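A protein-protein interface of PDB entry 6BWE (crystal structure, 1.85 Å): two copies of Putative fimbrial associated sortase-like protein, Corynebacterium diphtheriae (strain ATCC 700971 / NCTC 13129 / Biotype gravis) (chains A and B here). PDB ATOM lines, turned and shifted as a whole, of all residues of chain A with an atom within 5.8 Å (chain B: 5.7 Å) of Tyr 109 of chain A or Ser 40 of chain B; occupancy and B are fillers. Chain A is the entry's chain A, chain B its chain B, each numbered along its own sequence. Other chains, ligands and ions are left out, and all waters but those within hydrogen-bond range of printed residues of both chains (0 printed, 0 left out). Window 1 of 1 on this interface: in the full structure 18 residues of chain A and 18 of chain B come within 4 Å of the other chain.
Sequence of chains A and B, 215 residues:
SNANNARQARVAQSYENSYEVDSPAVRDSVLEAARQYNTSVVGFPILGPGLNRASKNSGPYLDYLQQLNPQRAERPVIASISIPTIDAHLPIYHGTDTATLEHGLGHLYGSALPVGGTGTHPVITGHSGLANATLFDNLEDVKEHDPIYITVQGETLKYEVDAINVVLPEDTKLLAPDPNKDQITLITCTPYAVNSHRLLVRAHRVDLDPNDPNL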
ATOM      1  N   TYR A  37     -25.728  18.640  29.368  1.00  0.00           N
ATOM      2  CA  TYR A  37     -25.274  17.308  28.975  1.00  0.00           C
ATOM      3  C   TYR A  37     -26.408  16.578  28.228  1.00  0.00           C
ATOM      4  O   TYR A  37     -26.203  16.048  27.124  1.00  0.00           O
ATOM      5  CB  TYR A  37     -24.765  16.481  30.175  1.00  0.00           C
ATOM      6  CG  TYR A  37     -24.517  15.043  29.809  1.00  0.00           C
ATOM      7  CD1 TYR A  37     -23.310  14.631  29.306  1.00  0.00           C
ATOM      8  CD2 TYR A  37     -25.557  14.113  29.865  1.00  0.00           C
ATOM      9  CE1 TYR A  37     -23.108  13.325  28.894  1.00  0.00           C
ATOM     10  CE2 TYR A  37     -25.370  12.804  29.457  1.00  0.00           C
ATOM     11  CZ  TYR A  37     -24.164  12.404  28.973  1.00  0.00           C
ATOM     12  OH  TYR A  37     -24.003  11.089  28.581  1.00  0.00           O
ATOM     13  N   PRO A  45     -30.443   3.928  24.316  1.00  0.00           N
ATOM     14  CA  PRO A  45     -29.597   2.742  24.326  1.00  0.00           C
ATOM     15  C   PRO A  45     -30.237   1.510  23.690  1.00  0.00           C
ATOM     16  O   PRO A  45     -31.290   1.094  24.120  1.00  0.00           O
ATOM     17  CB  PRO A  45     -29.311   2.507  25.824  1.00  0.00           C
ATOM     18  CG  PRO A  45     -29.923   3.650  26.545  1.00  0.00           C
ATOM     19  CD  PRO A  45     -30.946   4.262  25.654  1.00  0.00           C
ATOM     20  N   ALA A  54     -18.999   0.926  25.562  1.00  0.00           N
ATOM     21  CA  ALA A  54     -18.426   2.276  25.478  1.00  0.00           C
ATOM     22  C   ALA A  54     -17.104   2.314  26.187  1.00  0.00           C
ATOM     23  O   ALA A  54     -17.018   1.886  27.339  1.00  0.00           O
ATOM     24  CB  ALA A  54     -19.362   3.312  26.095  1.00  0.00           C
ATOM     25  N   SER A  55     -16.073   2.818  25.521  1.00  0.00           N
ATOM     26  CA  SER A  55     -14.807   2.992  26.183  1.00  0.00           C
ATOM     27  C   SER A  55     -15.097   4.067  27.224  1.00  0.00           C
ATOM     28  O   SER A  55     -15.749   5.077  26.917  1.00  0.00           O
ATOM     29  CB  SER A  55     -13.712   3.429  25.231  1.00  0.00           C
ATOM     30  OG  SER A  55     -12.621   3.954  25.937  1.00  0.00           O
ATOM     31  N   SER A  58     -13.368   7.560  26.449  1.00  0.00           N
ATOM     32  CA  SER A  58     -13.849   8.514  25.442  1.00  0.00           C
ATOM     33  C   SER A  58     -14.214   9.858  26.077  1.00  0.00           C
ATOM     34  O   SER A  58     -14.642   9.911  27.252  1.00  0.00           O
ATOM     35  CB  SER A  58     -15.024   7.896  24.668  1.00  0.00           C
ATOM     36  OG  SER A  58     -16.208   7.882  25.439  1.00  0.00           O
ATOM     37  N   PRO A  60     -16.884  11.752  25.581  1.00  0.00           N
ATOM     38  CA  PRO A  60     -18.270  11.825  26.087  1.00  0.00           C
ATOM     39  C   PRO A  60     -18.496  11.033  27.356  1.00  0.00           C
ATOM     40  O   PRO A  60     -19.270  11.495  28.200  1.00  0.00           O
ATOM     41  CB  PRO A  60     -19.095  11.239  24.934  1.00  0.00           C
ATOM     42  CG  PRO A  60     -18.286  11.618  23.716  1.00  0.00           C
ATOM     43  CD  PRO A  60     -16.864  11.401  24.147  1.00  0.00           C
ATOM     44  N   TYR A  61     -17.872   9.854  27.477  1.00  0.00           N
ATOM     45  CA  TYR A  61     -18.069   9.057  28.688  1.00  0.00           C
ATOM     46  C   TYR A  61     -17.429   9.752  29.907  1.00  0.00           C
ATOM     47  O   TYR A  61     -18.020   9.815  30.983  1.00  0.00           O
ATOM     48  CB  TYR A  61     -17.605   7.604  28.546  1.00  0.00           C
ATOM     49  CG  TYR A  61     -18.254   6.714  29.568  1.00  0.00           C
ATOM     50  CD1 TYR A  61     -17.665   6.512  30.829  1.00  0.00           C
ATOM     51  CD2 TYR A  61     -19.475   6.095  29.317  1.00  0.00           C
ATOM     52  CE1 TYR A  61     -18.253   5.713  31.776  1.00  0.00           C
ATOM     53  CE2 TYR A  61     -20.064   5.278  30.271  1.00  0.00           C
ATOM     54  CZ  TYR A  61     -19.447   5.102  31.502  1.00  0.00           C
ATOM     55  OH  TYR A  61     -20.011   4.275  32.453  1.00  0.00           O
ATOM     56  N   TYR A  64     -19.779  12.529  30.899  1.00  0.00           N
ATOM     57  CA  TYR A  64     -20.855  11.858  31.634  1.00  0.00           C
ATOM     58  C   TYR A  64     -20.527  11.643  33.117  1.00  0.00           C
ATOM     59  O   TYR A  64     -21.313  11.971  33.991  1.00  0.00           O
ATOM     60  CB  TYR A  64     -21.145  10.536  30.966  1.00  0.00           C
ATOM     61  CG  TYR A  64     -22.062   9.607  31.651  1.00  0.00           C
ATOM     62  CD1 TYR A  64     -23.432   9.894  31.776  1.00  0.00           C
ATOM     63  CD2 TYR A  64     -21.609   8.354  32.059  1.00  0.00           C
ATOM     64  CE1 TYR A  64     -24.288   8.953  32.344  1.00  0.00           C
ATOM     65  CE2 TYR A  64     -22.431   7.424  32.612  1.00  0.00           C
ATOM     66  CZ  TYR A  64     -23.760   7.727  32.802  1.00  0.00           C
ATOM     67  OH  TYR A  64     -24.578   6.750  33.341  1.00  0.00           O
ATOM     68  N   GLY A  95     -23.628   4.563  35.046  1.00  0.00           N
ATOM     69  CA  GLY A  95     -23.281   3.340  34.357  1.00  0.00           C
ATOM     70  C   GLY A  95     -23.954   2.100  34.875  1.00  0.00           C
ATOM     71  O   GLY A  95     -24.778   2.131  35.829  1.00  0.00           O
ATOM     72  N   THR A  96     -23.541   0.981  34.287  1.00  0.00           N
ATOM     73  CA  THR A  96     -24.158  -0.325  34.559  1.00  0.00           C
ATOM     74  C   THR A  96     -23.065  -1.380  34.699  1.00  0.00           C
ATOM     75  O   THR A  96     -23.252  -2.508  34.270  1.00  0.00           O
ATOM     76  CB  THR A  96     -25.179  -0.715  33.438  1.00  0.00           C
ATOM     77  OG1 THR A  96     -24.547  -0.617  32.156  1.00  0.00           O
ATOM     78  CG2 THR A  96     -26.334   0.195  33.481  1.00  0.00           C
ATOM     79  N   HIS A 107     -27.509   3.821  36.009  1.00  0.00           N
ATOM     80  CA  HIS A 107     -28.060   4.660  34.957  1.00  0.00           C
ATOM     81  C   HIS A 107     -27.487   4.181  33.623  1.00  0.00           C
ATOM     82  O   HIS A 107     -26.274   3.995  33.513  1.00  0.00           O
ATOM     83  CB  HIS A 107     -27.751   6.137  35.196  1.00  0.00           C
ATOM     84  CG  HIS A 107     -28.084   6.993  34.025  1.00  0.00           C
ATOM     85  ND1 HIS A 107     -27.147   7.357  33.082  1.00  0.00           N
ATOM     86  CD2 HIS A 107     -29.273   7.489  33.601  1.00  0.00           C
ATOM     87  CE1 HIS A 107     -27.747   8.066  32.133  1.00  0.00           C
ATOM     88  NE2 HIS A 107     -29.042   8.130  32.413  1.00  0.00           N
ATOM     89  N   LEU A 108     -28.357   3.967  32.628  1.00  0.00           N
ATOM     90  CA  LEU A 108     -27.914   3.490  31.331  1.00  0.00           C
ATOM     91  C   LEU A 108     -27.335   4.620  30.483  1.00  0.00           C
ATOM     92  O   LEU A 108     -28.061   5.495  30.002  1.00  0.00           O
ATOM     93  CB  LEU A 108     -29.061   2.777  30.618  1.00  0.00           C
ATOM     94  CG  LEU A 108     -28.782   1.885  29.424  1.00  0.00           C
ATOM     95  CD1 LEU A 108     -27.625   0.913  29.630  1.00  0.00           C
ATOM     96  CD2 LEU A 108     -30.051   1.126  29.086  1.00  0.00           C
ATOM     97  N   TYR A 109     -26.018   4.604  30.332  1.00  0.00           N
ATOM     98  CA  TYR A 109     -25.312   5.517  29.485  1.00  0.00           C
ATOM     99  C   TYR A 109     -25.940   5.514  28.072  1.00  0.00           C
ATOM    100  O   TYR A 109     -26.231   4.442  27.510  1.00  0.00           O
ATOM    101  CB  TYR A 109     -23.815   5.125  29.407  1.00  0.00           C
ATOM    102  CG  TYR A 109     -23.093   6.058  28.452  1.00  0.00           C
ATOM    103  CD1 TYR A 109     -22.875   7.392  28.786  1.00  0.00           C
ATOM    104  CD2 TYR A 109     -22.708   5.610  27.189  1.00  0.00           C
ATOM    105  CE1 TYR A 109     -22.251   8.260  27.876  1.00  0.00           C
ATOM    106  CE2 TYR A 109     -22.104   6.450  26.291  1.00  0.00           C
ATOM    107  CZ  TYR A 109     -21.896   7.769  26.617  1.00  0.00           C
ATOM    108  OH  TYR A 109     -21.297   8.552  25.660  1.00  0.00           O
ATOM    109  N   GLY A 110     -26.166   6.695  27.531  1.00  0.00           N
ATOM    110  CA  GLY A 110     -26.871   6.844  26.258  1.00  0.00           C
ATOM    111  C   GLY A 110     -28.314   7.274  26.403  1.00  0.00           C
ATOM    112  O   GLY A 110     -29.009   7.454  25.385  1.00  0.00           O
ATOM    113  N   SER A 111     -28.780   7.363  27.653  1.00  0.00           N
ATOM    114  CA  SER A 111     -30.061   7.948  27.986  1.00  0.00           C
ATOM    115  C   SER A 111     -29.772   9.199  28.814  1.00  0.00           C
ATOM    116  O   SER A 111     -28.682   9.348  29.364  1.00  0.00           O
ATOM    117  CB  SER A 111     -30.962   6.962  28.744  1.00  0.00           C
ATOM    118  OG  SER A 111     -30.441   6.654  30.058  1.00  0.00           O
ATOM    119  N   GLN B  36     -12.322   5.773  18.951  1.00  0.00           N
ATOM    120  CA  GLN B  36     -12.605   5.839  20.360  1.00  0.00           C
ATOM    121  C   GLN B  36     -13.846   6.707  20.624  1.00  0.00           C
ATOM    122  O   GLN B  36     -14.683   6.311  21.412  1.00  0.00           O
ATOM    123  CB  GLN B  36     -11.390   6.345  21.169  1.00  0.00           C
ATOM    124  CG  GLN B  36     -11.682   6.342  22.683  1.00  0.00           C
ATOM    125  CD  GLN B  36     -10.557   6.944  23.506  1.00  0.00           C
ATOM    126  OE1 GLN B  36     -10.076   6.333  24.456  1.00  0.00           O
ATOM    127  NE2 GLN B  36     -10.140   8.150  23.144  1.00  0.00           N
ATOM    128  N   TYR B  37     -13.964   7.852  19.940  1.00  0.00           N
ATOM    129  CA  TYR B  37     -15.163   8.681  20.038  1.00  0.00           C
ATOM    130  C   TYR B  37     -16.393   7.807  19.695  1.00  0.00           C
ATOM    131  O   TYR B  37     -17.389   7.825  20.404  1.00  0.00           O
ATOM    132  CB  TYR B  37     -15.090   9.955  19.149  1.00  0.00           C
ATOM    133  CG  TYR B  37     -16.443  10.608  19.040  1.00  0.00           C
ATOM    134  CD1 TYR B  37     -16.848  11.563  19.962  1.00  0.00           C
ATOM    135  CD2 TYR B  37     -17.356  10.227  18.026  1.00  0.00           C
ATOM    136  CE1 TYR B  37     -18.116  12.099  19.935  1.00  0.00           C
ATOM    137  CE2 TYR B  37     -18.642  10.777  17.970  1.00  0.00           C
ATOM    138  CZ  TYR B  37     -19.016  11.719  18.914  1.00  0.00           C
ATOM    139  OH  TYR B  37     -20.255  12.256  18.870  1.00  0.00           O
ATOM    140  N   ASN B  38     -16.283   7.011  18.639  1.00  0.00           N
ATOM    141  CA  ASN B  38     -17.417   6.201  18.173  1.00  0.00           C
ATOM    142  C   ASN B  38     -17.922   5.190  19.189  1.00  0.00           C
ATOM    143  O   ASN B  38     -19.103   4.880  19.202  1.00  0.00           O
ATOM    144  CB  ASN B  38     -17.076   5.502  16.838  1.00  0.00           C
ATOM    145  CG  ASN B  38     -17.140   6.455  15.656  1.00  0.00           C
ATOM    146  OD1 ASN B  38     -17.656   7.560  15.786  1.00  0.00           O
ATOM    147  ND2 ASN B  38     -16.613   6.029  14.491  1.00  0.00           N
ATOM    148  N   THR B  39     -17.053   4.704  20.074  1.00  0.00           N
ATOM    149  CA  THR B  39     -17.484   3.750  21.109  1.00  0.00           C
ATOM    150  C   THR B  39     -18.467   4.402  22.091  1.00  0.00           C
ATOM    151  O   THR B  39     -19.220   3.704  22.766  1.00  0.00           O
ATOM    152  CB  THR B  39     -16.315   3.182  21.947  1.00  0.00           C
ATOM    153  OG1 THR B  39     -15.712   4.225  22.751  1.00  0.00           O
ATOM    154  CG2 THR B  39     -15.269   2.519  21.071  1.00  0.00           C
ATOM    155  N   SER B  40     -18.462   5.739  22.159  1.00  0.00           N
ATOM    156  CA  SER B  40     -19.380   6.490  23.000  1.00  0.00           C
ATOM    157  C   SER B  40     -20.771   6.690  22.387  1.00  0.00           C
ATOM    158  O   SER B  40     -21.664   7.156  23.074  1.00  0.00           O
ATOM    159  CB  SER B  40     -18.769   7.858  23.318  1.00  0.00           C
ATOM    160  OG  SER B  40     -19.035   8.800  22.295  1.00  0.00           O
ATOM    161  N   VAL B  41     -20.945   6.335  21.112  1.00  0.00           N
ATOM    162  CA  VAL B  41     -22.192   6.564  20.410  1.00  0.00           C
ATOM    163  C   VAL B  41     -23.091   5.375  20.620  1.00  0.00           C
ATOM    164  O   VAL B  41     -22.781   4.282  20.185  1.00  0.00           O
ATOM    165  CB  VAL B  41     -21.921   6.783  18.912  1.00  0.00           C
ATOM    166  CG1 VAL B  41     -23.237   6.877  18.129  1.00  0.00           C
ATOM    167  CG2 VAL B  41     -21.071   8.043  18.746  1.00  0.00           C
ATOM    168  N   VAL B  42     -24.217   5.574  21.271  1.00  0.00           N
ATOM    169  CA  VAL B  42     -24.939   4.429  21.798  1.00  0.00           C
ATOM    170  C   VAL B  42     -26.212   4.064  21.050  1.00  0.00           C
ATOM    171  O   VAL B  42     -26.672   2.926  21.107  1.00  0.00           O
ATOM    172  CB  VAL B  42     -25.136   4.612  23.351  1.00  0.00           C
ATOM    173  CG1 VAL B  42     -26.426   4.047  23.842  1.00  0.00           C
ATOM    174  CG2 VAL B  42     -23.963   3.942  24.031  1.00  0.00           C
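The backbone NH (N) of Ser 55 of chain A is in hydrogen-bond range of the side-chain hydroxyl (OG1) of Thr 39 of chain B (3.1 Å). The side-chain hydroxyl of Tyr 109 of chain A is in hydrogen-bond range of the backbone carbonyl oxygen of Ser 40 of chain B (3.0 Å).
O of Gln 36 of chain B lies within hydrogen-bond range of OG1 of Thr 39 of chain B (2.7 Å). O of Tyr 37 of chain B lies within hydrogen-bond range of OG of Ser 40 of chain B (2.7 Å). N of Tyr 61 of chain A sits at hydrogen-bond distance from OG of Ser 58 of chain A (3.3 Å). The backbone carbonyl oxygen of Ser 55 of chain A sits at hydrogen-bond distance from the side-chain hydroxyl of Ser 58 of chain A, at 3.2 Å.
CG1 of Val 42 of chain B touches CA of Pro 45 of chain A, 3.5 Å away. CA of Ala 54 of chain A touches O of Thr 39 of chain B (3.2 Å). Ser 55 of chain A touches Gln 36 of chain B. O of Gln 36 of chain B touches CB of Ser 58 of chain A, at 3.6 Å. Ser 40 of chain B touches Ser 58 of chain A. Pro 60 of chain A touches Tyr 37 of chain B. Pro 60 of chain A touches Ser 40 of chain B (CG to OG, 3.2 Å). Tyr 109 of chain A touches Val 42 of chain B. Gly 110 of chain A touches Val 42 of chain B.
Printed residues of chain B within 4 Å of Ser 58 of chain A: Gln 36 (3.6 Å) and Ser 40 (3.3 Å). Tyr 109 of chain A touches just these residues of chain B: Ser 40 and Val 42. Printed residues of chain B within 4 Å of Gly 110 of chain A: Val 42 (3.7 Å). Asn 38 of chain B touches none of the printed residues of chain A. Ser 40 of chain B touches just these residues of chain A: Ser 58, Pro 60 and Tyr 109. The nearest residue of chain B that does not touch Tyr 109 of chain A is Val 41 of chain B (5.1 Å). The nearest residue of chain A that does not touch Ser 40 of chain B is Ala 54 of chain A (4.4 Å).
Hydrophobic or aromatic side chains of chain B that line the printed part of chain A: Tyr 37 and Val 42. Hydrophobic or aromatic side chains of chain A within 4 Å of the printed part of chain B: Pro 45, Ala 54, Pro 60 and Tyr 109.
1 position is printed for both chains. Of the 11 pairs that touch across the chains among the printed residues, none has its exchanged pair printed and touching as well.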
